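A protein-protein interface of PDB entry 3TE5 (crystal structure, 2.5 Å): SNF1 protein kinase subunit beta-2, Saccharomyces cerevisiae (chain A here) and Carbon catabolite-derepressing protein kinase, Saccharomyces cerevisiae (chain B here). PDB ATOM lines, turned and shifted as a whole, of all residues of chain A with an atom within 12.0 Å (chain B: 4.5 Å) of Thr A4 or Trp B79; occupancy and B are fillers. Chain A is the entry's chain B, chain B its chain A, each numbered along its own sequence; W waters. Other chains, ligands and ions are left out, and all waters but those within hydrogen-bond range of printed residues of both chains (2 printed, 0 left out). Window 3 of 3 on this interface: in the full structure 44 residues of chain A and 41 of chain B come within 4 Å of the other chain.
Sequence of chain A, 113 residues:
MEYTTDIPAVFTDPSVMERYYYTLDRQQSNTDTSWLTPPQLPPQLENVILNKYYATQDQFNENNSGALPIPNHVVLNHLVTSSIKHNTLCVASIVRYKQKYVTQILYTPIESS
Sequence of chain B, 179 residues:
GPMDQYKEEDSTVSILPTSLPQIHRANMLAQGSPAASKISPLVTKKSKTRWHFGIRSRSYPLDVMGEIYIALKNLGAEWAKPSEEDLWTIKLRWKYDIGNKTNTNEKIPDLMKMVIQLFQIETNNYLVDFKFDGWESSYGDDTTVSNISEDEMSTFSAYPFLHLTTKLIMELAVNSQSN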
ATOM      1  N   MET A   1     -12.109   4.246  38.819  1.00  0.00           N
ATOM      2  CA  MET A   1     -12.250   4.668  37.394  1.00  0.00           C
ATOM      3  C   MET A   1     -12.273   3.465  36.452  1.00  0.00           C
ATOM      4  O   MET A   1     -11.740   2.401  36.776  1.00  0.00           O
ATOM      5  CB  MET A   1     -11.115   5.621  37.008  1.00  0.00           C
ATOM      6  N   GLU A   2     -12.900   3.640  35.292  1.00  0.00           N
ATOM      7  CA  GLU A   2     -12.907   2.615  34.250  1.00  0.00           C
ATOM      8  C   GLU A   2     -11.800   2.887  33.231  1.00  0.00           C
ATOM      9  O   GLU A   2     -11.627   4.021  32.778  1.00  0.00           O
ATOM     10  CB  GLU A   2     -14.272   2.553  33.559  1.00  0.00           C
ATOM     11  N   TYR A   3     -11.055   1.842  32.878  1.00  0.00           N
ATOM     12  CA  TYR A   3      -9.913   1.968  31.972  1.00  0.00           C
ATOM     13  C   TYR A   3     -10.166   1.284  30.636  1.00  0.00           C
ATOM     14  O   TYR A   3     -10.678   0.164  30.589  1.00  0.00           O
ATOM     15  CB  TYR A   3      -8.647   1.391  32.617  1.00  0.00           C
ATOM     16  CG  TYR A   3      -8.029   2.261  33.694  1.00  0.00           C
ATOM     17  CD1 TYR A   3      -6.981   3.129  33.395  1.00  0.00           C
ATOM     18  CD2 TYR A   3      -8.485   2.210  35.012  1.00  0.00           C
ATOM     19  CE1 TYR A   3      -6.405   3.929  34.378  1.00  0.00           C
ATOM     20  CE2 TYR A   3      -7.914   3.005  36.003  1.00  0.00           C
ATOM     21  CZ  TYR A   3      -6.875   3.860  35.679  1.00  0.00           C
ATOM     22  OH  TYR A   3      -6.306   4.650  36.653  1.00  0.00           O
ATOM     23  N   THR A   4      -9.814   1.973  29.552  1.00  0.00           N
ATOM     24  CA  THR A   4      -9.909   1.417  28.195  1.00  0.00           C
ATOM     25  C   THR A   4      -8.875   2.035  27.245  1.00  0.00           C
ATOM     26  O   THR A   4      -8.257   3.056  27.564  1.00  0.00           O
ATOM     27  CB  THR A   4     -11.366   1.468  27.593  1.00  0.00           C
ATOM     28  OG1 THR A   4     -11.323   1.953  26.245  1.00  0.00           O
ATOM     29  CG2 THR A   4     -12.301   2.361  28.407  1.00  0.00           C
ATOM     30  N   THR A   5      -8.697   1.399  26.088  1.00  0.00           N
ATOM     31  CA  THR A   5      -7.693   1.802  25.101  1.00  0.00           C
ATOM     32  C   THR A   5      -8.269   2.710  24.006  1.00  0.00           C
ATOM     33  O   THR A   5      -7.657   2.893  22.947  1.00  0.00           O
ATOM     34  CB  THR A   5      -7.027   0.568  24.442  1.00  0.00           C
ATOM     35  OG1 THR A   5      -7.965  -0.081  23.575  1.00  0.00           O
ATOM     36  CG2 THR A   5      -6.547  -0.425  25.497  1.00  0.00           C
ATOM     37  N   ASP A   6      -9.441   3.282  24.269  1.00  0.00           N
ATOM     38  CA  ASP A   6     -10.103   4.163  23.306  1.00  0.00           C
ATOM     39  C   ASP A   6      -9.706   5.620  23.526  1.00  0.00           C
ATOM     40  O   ASP A   6     -10.021   6.212  24.561  1.00  0.00           O
ATOM     41  CB  ASP A   6     -11.626   3.995  23.376  1.00  0.00           C
ATOM     42  CG  ASP A   6     -12.076   2.598  22.989  1.00  0.00           C
ATOM     43  OD1 ASP A   6     -11.637   2.096  21.930  1.00  0.00           O
ATOM     44  OD2 ASP A   6     -12.872   2.002  23.745  1.00  0.00           O
ATOM     45  N   ILE A   7      -9.004   6.182  22.545  1.00  0.00           N
ATOM     46  CA  ILE A   7      -8.550   7.568  22.601  1.00  0.00           C
ATOM     47  C   ILE A   7      -9.751   8.511  22.701  1.00  0.00           C
ATOM     48  O   ILE A   7     -10.674   8.421  21.884  1.00  0.00           O
ATOM     49  CB  ILE A   7      -7.679   7.936  21.370  1.00  0.00           C
ATOM     50  CG1 ILE A   7      -6.495   6.969  21.240  1.00  0.00           C
ATOM     51  CG2 ILE A   7      -7.202   9.387  21.455  1.00  0.00           C
ATOM     52  CD1 ILE A   7      -5.749   7.054  19.924  1.00  0.00           C
ATOM     53  N   PRO A   8      -9.752   9.399  23.716  1.00  0.00           N
ATOM     54  CA  PRO A   8     -10.799  10.403  23.889  1.00  0.00           C
ATOM     55  C   PRO A   8     -11.079  11.155  22.589  1.00  0.00           C
ATOM     56  O   PRO A   8     -10.147  11.643  21.937  1.00  0.00           O
ATOM     57  CB  PRO A   8     -10.206  11.344  24.939  1.00  0.00           C
ATOM     58  CG  PRO A   8      -9.308  10.478  25.741  1.00  0.00           C
ATOM     59  CD  PRO A   8      -8.753   9.456  24.799  1.00  0.00           C
ATOM     60  N   ALA A   9     -12.362  11.235  22.231  1.00  0.00           N
ATOM     61  CA  ALA A   9     -12.808  11.780  20.941  1.00  0.00           C
ATOM     62  C   ALA A   9     -12.324  13.203  20.662  1.00  0.00           C
ATOM     63  O   ALA A   9     -12.078  13.558  19.510  1.00  0.00           O
ATOM     64  CB  ALA A   9     -14.327  11.700  20.829  1.00  0.00           C
ATOM     65  N   VAL A  10     -12.179  13.999  21.721  1.00  0.00           N
ATOM     66  CA  VAL A  10     -11.691  15.383  21.624  1.00  0.00           C
ATOM     67  C   VAL A  10     -10.352  15.528  20.873  1.00  0.00           C
ATOM     68  O   VAL A  10     -10.076  16.579  20.295  1.00  0.00           O
ATOM     69  CB  VAL A  10     -11.644  16.075  23.031  1.00  0.00           C
ATOM     70  CG1 VAL A  10     -10.679  15.361  23.976  1.00  0.00           C
ATOM     71  CG2 VAL A  10     -11.303  17.560  22.919  1.00  0.00           C
ATOM     72  N   PHE A  11      -9.539  14.472  20.871  1.00  0.00           N
ATOM     73  CA  PHE A  11      -8.243  14.497  20.181  1.00  0.00           C
ATOM     74  C   PHE A  11      -8.260  13.791  18.816  1.00  0.00           C
ATOM     75  O   PHE A  11      -7.255  13.802  18.099  1.00  0.00           O
ATOM     76  CB  PHE A  11      -7.134  13.913  21.071  1.00  0.00           C
ATOM     77  CG  PHE A  11      -7.142  14.437  22.482  1.00  0.00           C
ATOM     78  CD1 PHE A  11      -6.969  15.794  22.740  1.00  0.00           C
ATOM     79  CD2 PHE A  11      -7.321  13.568  23.556  1.00  0.00           C
ATOM     80  CE1 PHE A  11      -6.984  16.282  24.048  1.00  0.00           C
ATOM     81  CE2 PHE A  11      -7.333  14.045  24.868  1.00  0.00           C
ATOM     82  CZ  PHE A  11      -7.161  15.403  25.112  1.00  0.00           C
ATOM     83  N   THR A  12      -9.394  13.186  18.461  1.00  0.00           N
ATOM     84  CA  THR A  12      -9.522  12.464  17.187  1.00  0.00           C
ATOM     85  C   THR A  12     -10.636  13.000  16.288  1.00  0.00           C
ATOM     86  O   THR A  12     -10.628  12.766  15.083  1.00  0.00           O
ATOM     87  CB  THR A  12      -9.759  10.955  17.398  1.00  0.00           C
ATOM     88  OG1 THR A  12     -10.898  10.762  18.246  1.00  0.00           O
ATOM     89  CG2 THR A  12      -8.533  10.292  18.020  1.00  0.00           C
ATOM     90  N   TYR B  69      -1.319   9.938  23.018  1.00  0.00           N
ATOM     91  CA  TYR B  69      -2.265   8.824  23.055  1.00  0.00           C
ATOM     92  C   TYR B  69      -1.934   7.720  22.051  1.00  0.00           C
ATOM     93  O   TYR B  69      -2.033   6.533  22.376  1.00  0.00           O
ATOM     94  CB  TYR B  69      -3.700   9.319  22.857  1.00  0.00           C
ATOM     95  CG  TYR B  69      -4.372   9.762  24.138  1.00  0.00           C
ATOM     96  CD1 TYR B  69      -4.823   8.825  25.067  1.00  0.00           C
ATOM     97  CD2 TYR B  69      -4.556  11.113  24.424  1.00  0.00           C
ATOM     98  CE1 TYR B  69      -5.435   9.219  26.248  1.00  0.00           C
ATOM     99  CE2 TYR B  69      -5.170  11.518  25.604  1.00  0.00           C
ATOM    100  CZ  TYR B  69      -5.608  10.565  26.508  1.00  0.00           C
ATOM    101  OH  TYR B  69      -6.219  10.952  27.678  1.00  0.00           O
ATOM    102  N   LEU B  72       0.981   5.832  23.504  1.00  0.00           N
ATOM    103  CA  LEU B  72       0.410   5.008  24.570  1.00  0.00           C
ATOM    104  C   LEU B  72      -0.265   3.746  24.040  1.00  0.00           C
ATOM    105  O   LEU B  72      -0.033   2.648  24.554  1.00  0.00           O
ATOM    106  CB  LEU B  72      -0.599   5.823  25.392  1.00  0.00           C
ATOM    107  CG  LEU B  72      -0.190   6.491  26.713  1.00  0.00           C
ATOM    108  CD1 LEU B  72       1.009   7.400  26.569  1.00  0.00           C
ATOM    109  CD2 LEU B  72      -1.357   7.272  27.298  1.00  0.00           C
ATOM    110  N   LYS B  73      -1.096   3.911  23.010  1.00  0.00           N
ATOM    111  CA  LYS B  73      -1.861   2.807  22.437  1.00  0.00           C
ATOM    112  C   LYS B  73      -0.957   1.778  21.756  1.00  0.00           C
ATOM    113  O   LYS B  73      -1.140   0.572  21.937  1.00  0.00           O
ATOM    114  CB  LYS B  73      -2.925   3.331  21.465  1.00  0.00           C
ATOM    115  CG  LYS B  73      -3.915   2.273  20.974  1.00  0.00           C
ATOM    116  CD  LYS B  73      -5.130   2.912  20.304  1.00  0.00           C
ATOM    117  CE  LYS B  73      -5.934   1.898  19.493  1.00  0.00           C
ATOM    118  NZ  LYS B  73      -6.597   0.867  20.341  1.00  0.00           N
ATOM    119  N   ALA B  77      -0.718   0.523  26.492  1.00  0.00           N
ATOM    120  CA  ALA B  77      -1.240   1.113  27.727  1.00  0.00           C
ATOM    121  C   ALA B  77      -2.745   1.386  27.654  1.00  0.00           C
ATOM    122  O   ALA B  77      -3.326   1.447  26.568  1.00  0.00           O
ATOM    123  CB  ALA B  77      -0.478   2.389  28.071  1.00  0.00           C
ATOM    124  N   GLU B  78      -3.364   1.537  28.823  1.00  0.00           N
ATOM    125  CA  GLU B  78      -4.773   1.917  28.939  1.00  0.00           C
ATOM    126  C   GLU B  78      -4.891   3.189  29.779  1.00  0.00           C
ATOM    127  O   GLU B  78      -3.957   3.549  30.486  1.00  0.00           O
ATOM    128  CB  GLU B  78      -5.609   0.775  29.539  1.00  0.00           C
ATOM    129  CG  GLU B  78      -5.072   0.206  30.853  1.00  0.00           C
ATOM    130  CD  GLU B  78      -5.956  -0.884  31.448  1.00  0.00           C
ATOM    131  OE1 GLU B  78      -6.557  -1.672  30.682  1.00  0.00           O
ATOM    132  OE2 GLU B  78      -6.039  -0.955  32.693  1.00  0.00           O
ATOM    133  N   TRP B  79      -6.032   3.869  29.692  1.00  0.00           N
ATOM    134  CA  TRP B  79      -6.224   5.152  30.374  1.00  0.00           C
ATOM    135  C   TRP B  79      -7.689   5.407  30.722  1.00  0.00           C
ATOM    136  O   TRP B  79      -8.590   4.765  30.178  1.00  0.00           O
ATOM    137  CB  TRP B  79      -5.690   6.300  29.511  1.00  0.00           C
ATOM    138  CG  TRP B  79      -6.214   6.258  28.111  1.00  0.00           C
ATOM    139  CD1 TRP B  79      -7.392   6.782  27.660  1.00  0.00           C
ATOM    140  CD2 TRP B  79      -5.591   5.638  26.979  1.00  0.00           C
ATOM    141  NE1 TRP B  79      -7.539   6.533  26.318  1.00  0.00           N
ATOM    142  CE2 TRP B  79      -6.450   5.831  25.873  1.00  0.00           C
ATOM    143  CE3 TRP B  79      -4.392   4.939  26.791  1.00  0.00           C
ATOM    144  CZ2 TRP B  79      -6.145   5.353  24.594  1.00  0.00           C
ATOM    145  CZ3 TRP B  79      -4.090   4.462  25.519  1.00  0.00           C
ATOM    146  CH2 TRP B  79      -4.965   4.672  24.438  1.00  0.00           C
ATOM    147  N   ALA B  80      -7.915   6.353  31.630  1.00  0.00           N
ATOM    148  CA  ALA B  80      -9.263   6.748  32.022  1.00  0.00           C
ATOM    149  C   ALA B  80      -9.887   7.690  30.994  1.00  0.00           C
ATOM    150  O   ALA B  80      -9.186   8.265  30.158  1.00  0.00           O
ATOM    151  CB  ALA B  80      -9.239   7.405  33.394  1.00  0.00           C
ATOM    152  N   LYS B  81     -11.210   7.826  31.061  1.00  0.00           N
ATOM    153  CA  LYS B  81     -11.949   8.805  30.264  1.00  0.00           C
ATOM    154  C   LYS B  81     -11.900  10.167  30.972  1.00  0.00           C
ATOM    155  O   LYS B  81     -12.374  10.299  32.102  1.00  0.00           O
ATOM    156  CB  LYS B  81     -13.392   8.319  30.043  1.00  0.00           C
ATOM    157  CG  LYS B  81     -14.438   9.394  29.735  1.00  0.00           C
ATOM    158  CD  LYS B  81     -14.577   9.668  28.247  1.00  0.00           C
ATOM    159  CE  LYS B  81     -15.711  10.652  27.988  1.00  0.00           C
ATOM    160  NZ  LYS B  81     -15.809  11.018  26.550  1.00  0.00           N
ATOM    161  N   ILE B  90      -3.770  13.011  31.536  1.00  0.00           N
ATOM    162  CA  ILE B  90      -3.958  11.606  31.200  1.00  0.00           C
ATOM    163  C   ILE B  90      -3.674  10.743  32.424  1.00  0.00           C
ATOM    164  O   ILE B  90      -2.549  10.703  32.926  1.00  0.00           O
ATOM    165  CB  ILE B  90      -3.081  11.153  30.007  1.00  0.00           C
ATOM    166  CG1 ILE B  90      -3.273  12.090  28.808  1.00  0.00           C
ATOM    167  CG2 ILE B  90      -3.408   9.706  29.628  1.00  0.00           C
ATOM    168  CD1 ILE B  90      -2.186  12.002  27.756  1.00  0.00           C
ATOM    169  N   LYS B  91      -4.718  10.078  32.909  1.00  0.00           N
ATOM    170  CA  LYS B  91      -4.603   9.128  34.001  1.00  0.00           C
ATOM    171  C   LYS B  91      -4.544   7.747  33.374  1.00  0.00           C
ATOM    172  O   LYS B  91      -5.570   7.185  32.979  1.00  0.00           O
ATOM    173  CB  LYS B  91      -5.790   9.258  34.958  1.00  0.00           C
ATOM    174  CG  LYS B  91      -5.862  10.608  35.661  1.00  0.00           C
ATOM    175  CD  LYS B  91      -7.256  10.889  36.200  1.00  0.00           C
ATOM    176  CE  LYS B  91      -7.383  12.336  36.659  1.00  0.00           C
ATOM    177  NZ  LYS B  91      -8.802  12.722  36.872  1.00  0.00           N
ATOM    178  N   LEU B  92      -3.332   7.215  33.265  1.00  0.00           N
ATOM    179  CA  LEU B  92      -3.100   5.993  32.511  1.00  0.00           C
ATOM    180  C   LEU B  92      -2.621   4.832  33.372  1.00  0.00           C
ATOM    181  O   LEU B  92      -2.219   5.009  34.523  1.00  0.00           O
ATOM    182  CB  LEU B  92      -2.122   6.253  31.359  1.00  0.00           C
ATOM    183  CG  LEU B  92      -0.650   6.492  31.704  1.00  0.00           C
ATOM    184  CD1 LEU B  92       0.191   5.258  31.402  1.00  0.00           C
ATOM    185  CD2 LEU B  92      -0.128   7.677  30.930  1.00  0.00           C
HETATM  186  O   HOH W   1     -14.206  10.367  24.085  1.00  0.00           O
HETATM  187  O   HOH W   2      -3.982   6.213  36.385  1.00  0.00           O
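Water W1 bridges N of Ala A9 (2.8 Å) and NZ of Lys B81 (3.0 Å).
Water W2 bridges the side-chain hydroxyl of Tyr A3 (2.8 Å) and the backbone carbonyl oxygen of Leu B92 (2.8 Å).
Of the 12 printed residues of chain A, 8 touch a printed residue of chain B.
Hydrophobic or aromatic side chains of chain B within 4 Å of the printed part of chain A: Tyr B69 and Trp B79.
Along chain B the printed residues that touch a printed residue of chain A span positions 69 to 91.
Among the printed residues, no Asp or Glu carboxylate lies within 4 Å of a Lys or Arg side-chain nitrogen of the other chain.
Among the printed residues, merely in contact across the chains: Glu A2 with Ala B80 (3.7 Å), Tyr A3 with Glu B78 (3.5 Å), Tyr A3 with Trp B79 (3.6 Å), Tyr A3 with Ala B80 (3.8 Å), Tyr A3 with Lys B91 (3.6 Å), Thr A4 with Glu B78 (3.9 Å), Thr A5 with Ala B77 (3.9 Å), Thr A5 with Trp B79 (3.3 Å), Ile A7 with Tyr B69 (3.8 Å), Ile A7 with Trp B79 (3.6 Å), Pro A8 with Tyr B69 (3.6 Å), Pro A8 with Trp B79 (3.5 Å) and Phe A11 with Tyr B69 (3.4 Å).
Trp B79 touches just these residues of chain A: Tyr A3 (3.6 Å), Thr A4 (3.1 Å), Thr A5 (3.3 Å), Asp A6 (3.1 Å), Ile A7 (3.6 Å) and Pro A8 (3.5 Å).
Tyr B69 touches just these residues of chain A: Ile A7, Pro A8 and Phe A11.
Of the printed residues of chain A, Lys B73 touches Thr A5 (3.5 Å).
Of chain A, only Thr A5 comes within 4 Å of Ala B77.
Glu B78 touches just these residues of chain A: Tyr A3 (3.5 Å) and Thr A4 (3.9 Å).
Of the printed residues of chain A, Ala B80 touches Glu A2 (3.7 Å) and Tyr A3 (3.8 Å).
No residue of chain A comes within 4 Å of Ile B90.
Printed residues of chain B within 4 Å of Tyr A3: Glu B78 (3.5 Å), Trp B79 (3.6 Å), Ala B80 (3.8 Å) and Lys B91 (3.6 Å).
Of the printed residues of chain B, Asp A6 touches Trp B79 (3.1 Å).
Thr A12 touches none of the printed residues of chain B.
Met A1 touches none of the printed residues of chain B.
The nearest residue of chain A that does not touch Trp B79 is Glu A2 (4.1 Å).
NZ of Lys B73 sits at hydrogen-bond distance from O of Thr A5, at 3.5 Å.
The backbone carbonyl oxygen (O) of Trp B79 sits at hydrogen-bond distance from the backbone NH (N) of Thr A4 (3.1 Å).
O of Asp A6 lies within hydrogen-bond range of NE1 of Trp B79.
The backbone carbonyl oxygen of Leu B72 is in hydrogen-bond range of the backbone NH of Ala B77.
N of Ala B80 is in hydrogen-bond range of O of Lys B91 (2.8 Å).
The side-chain hydroxyl (OG1) of Thr A4 sits at hydrogen-bond distance from the side-chain carboxylate (OD2) of Asp A6, at 2.9 Å.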
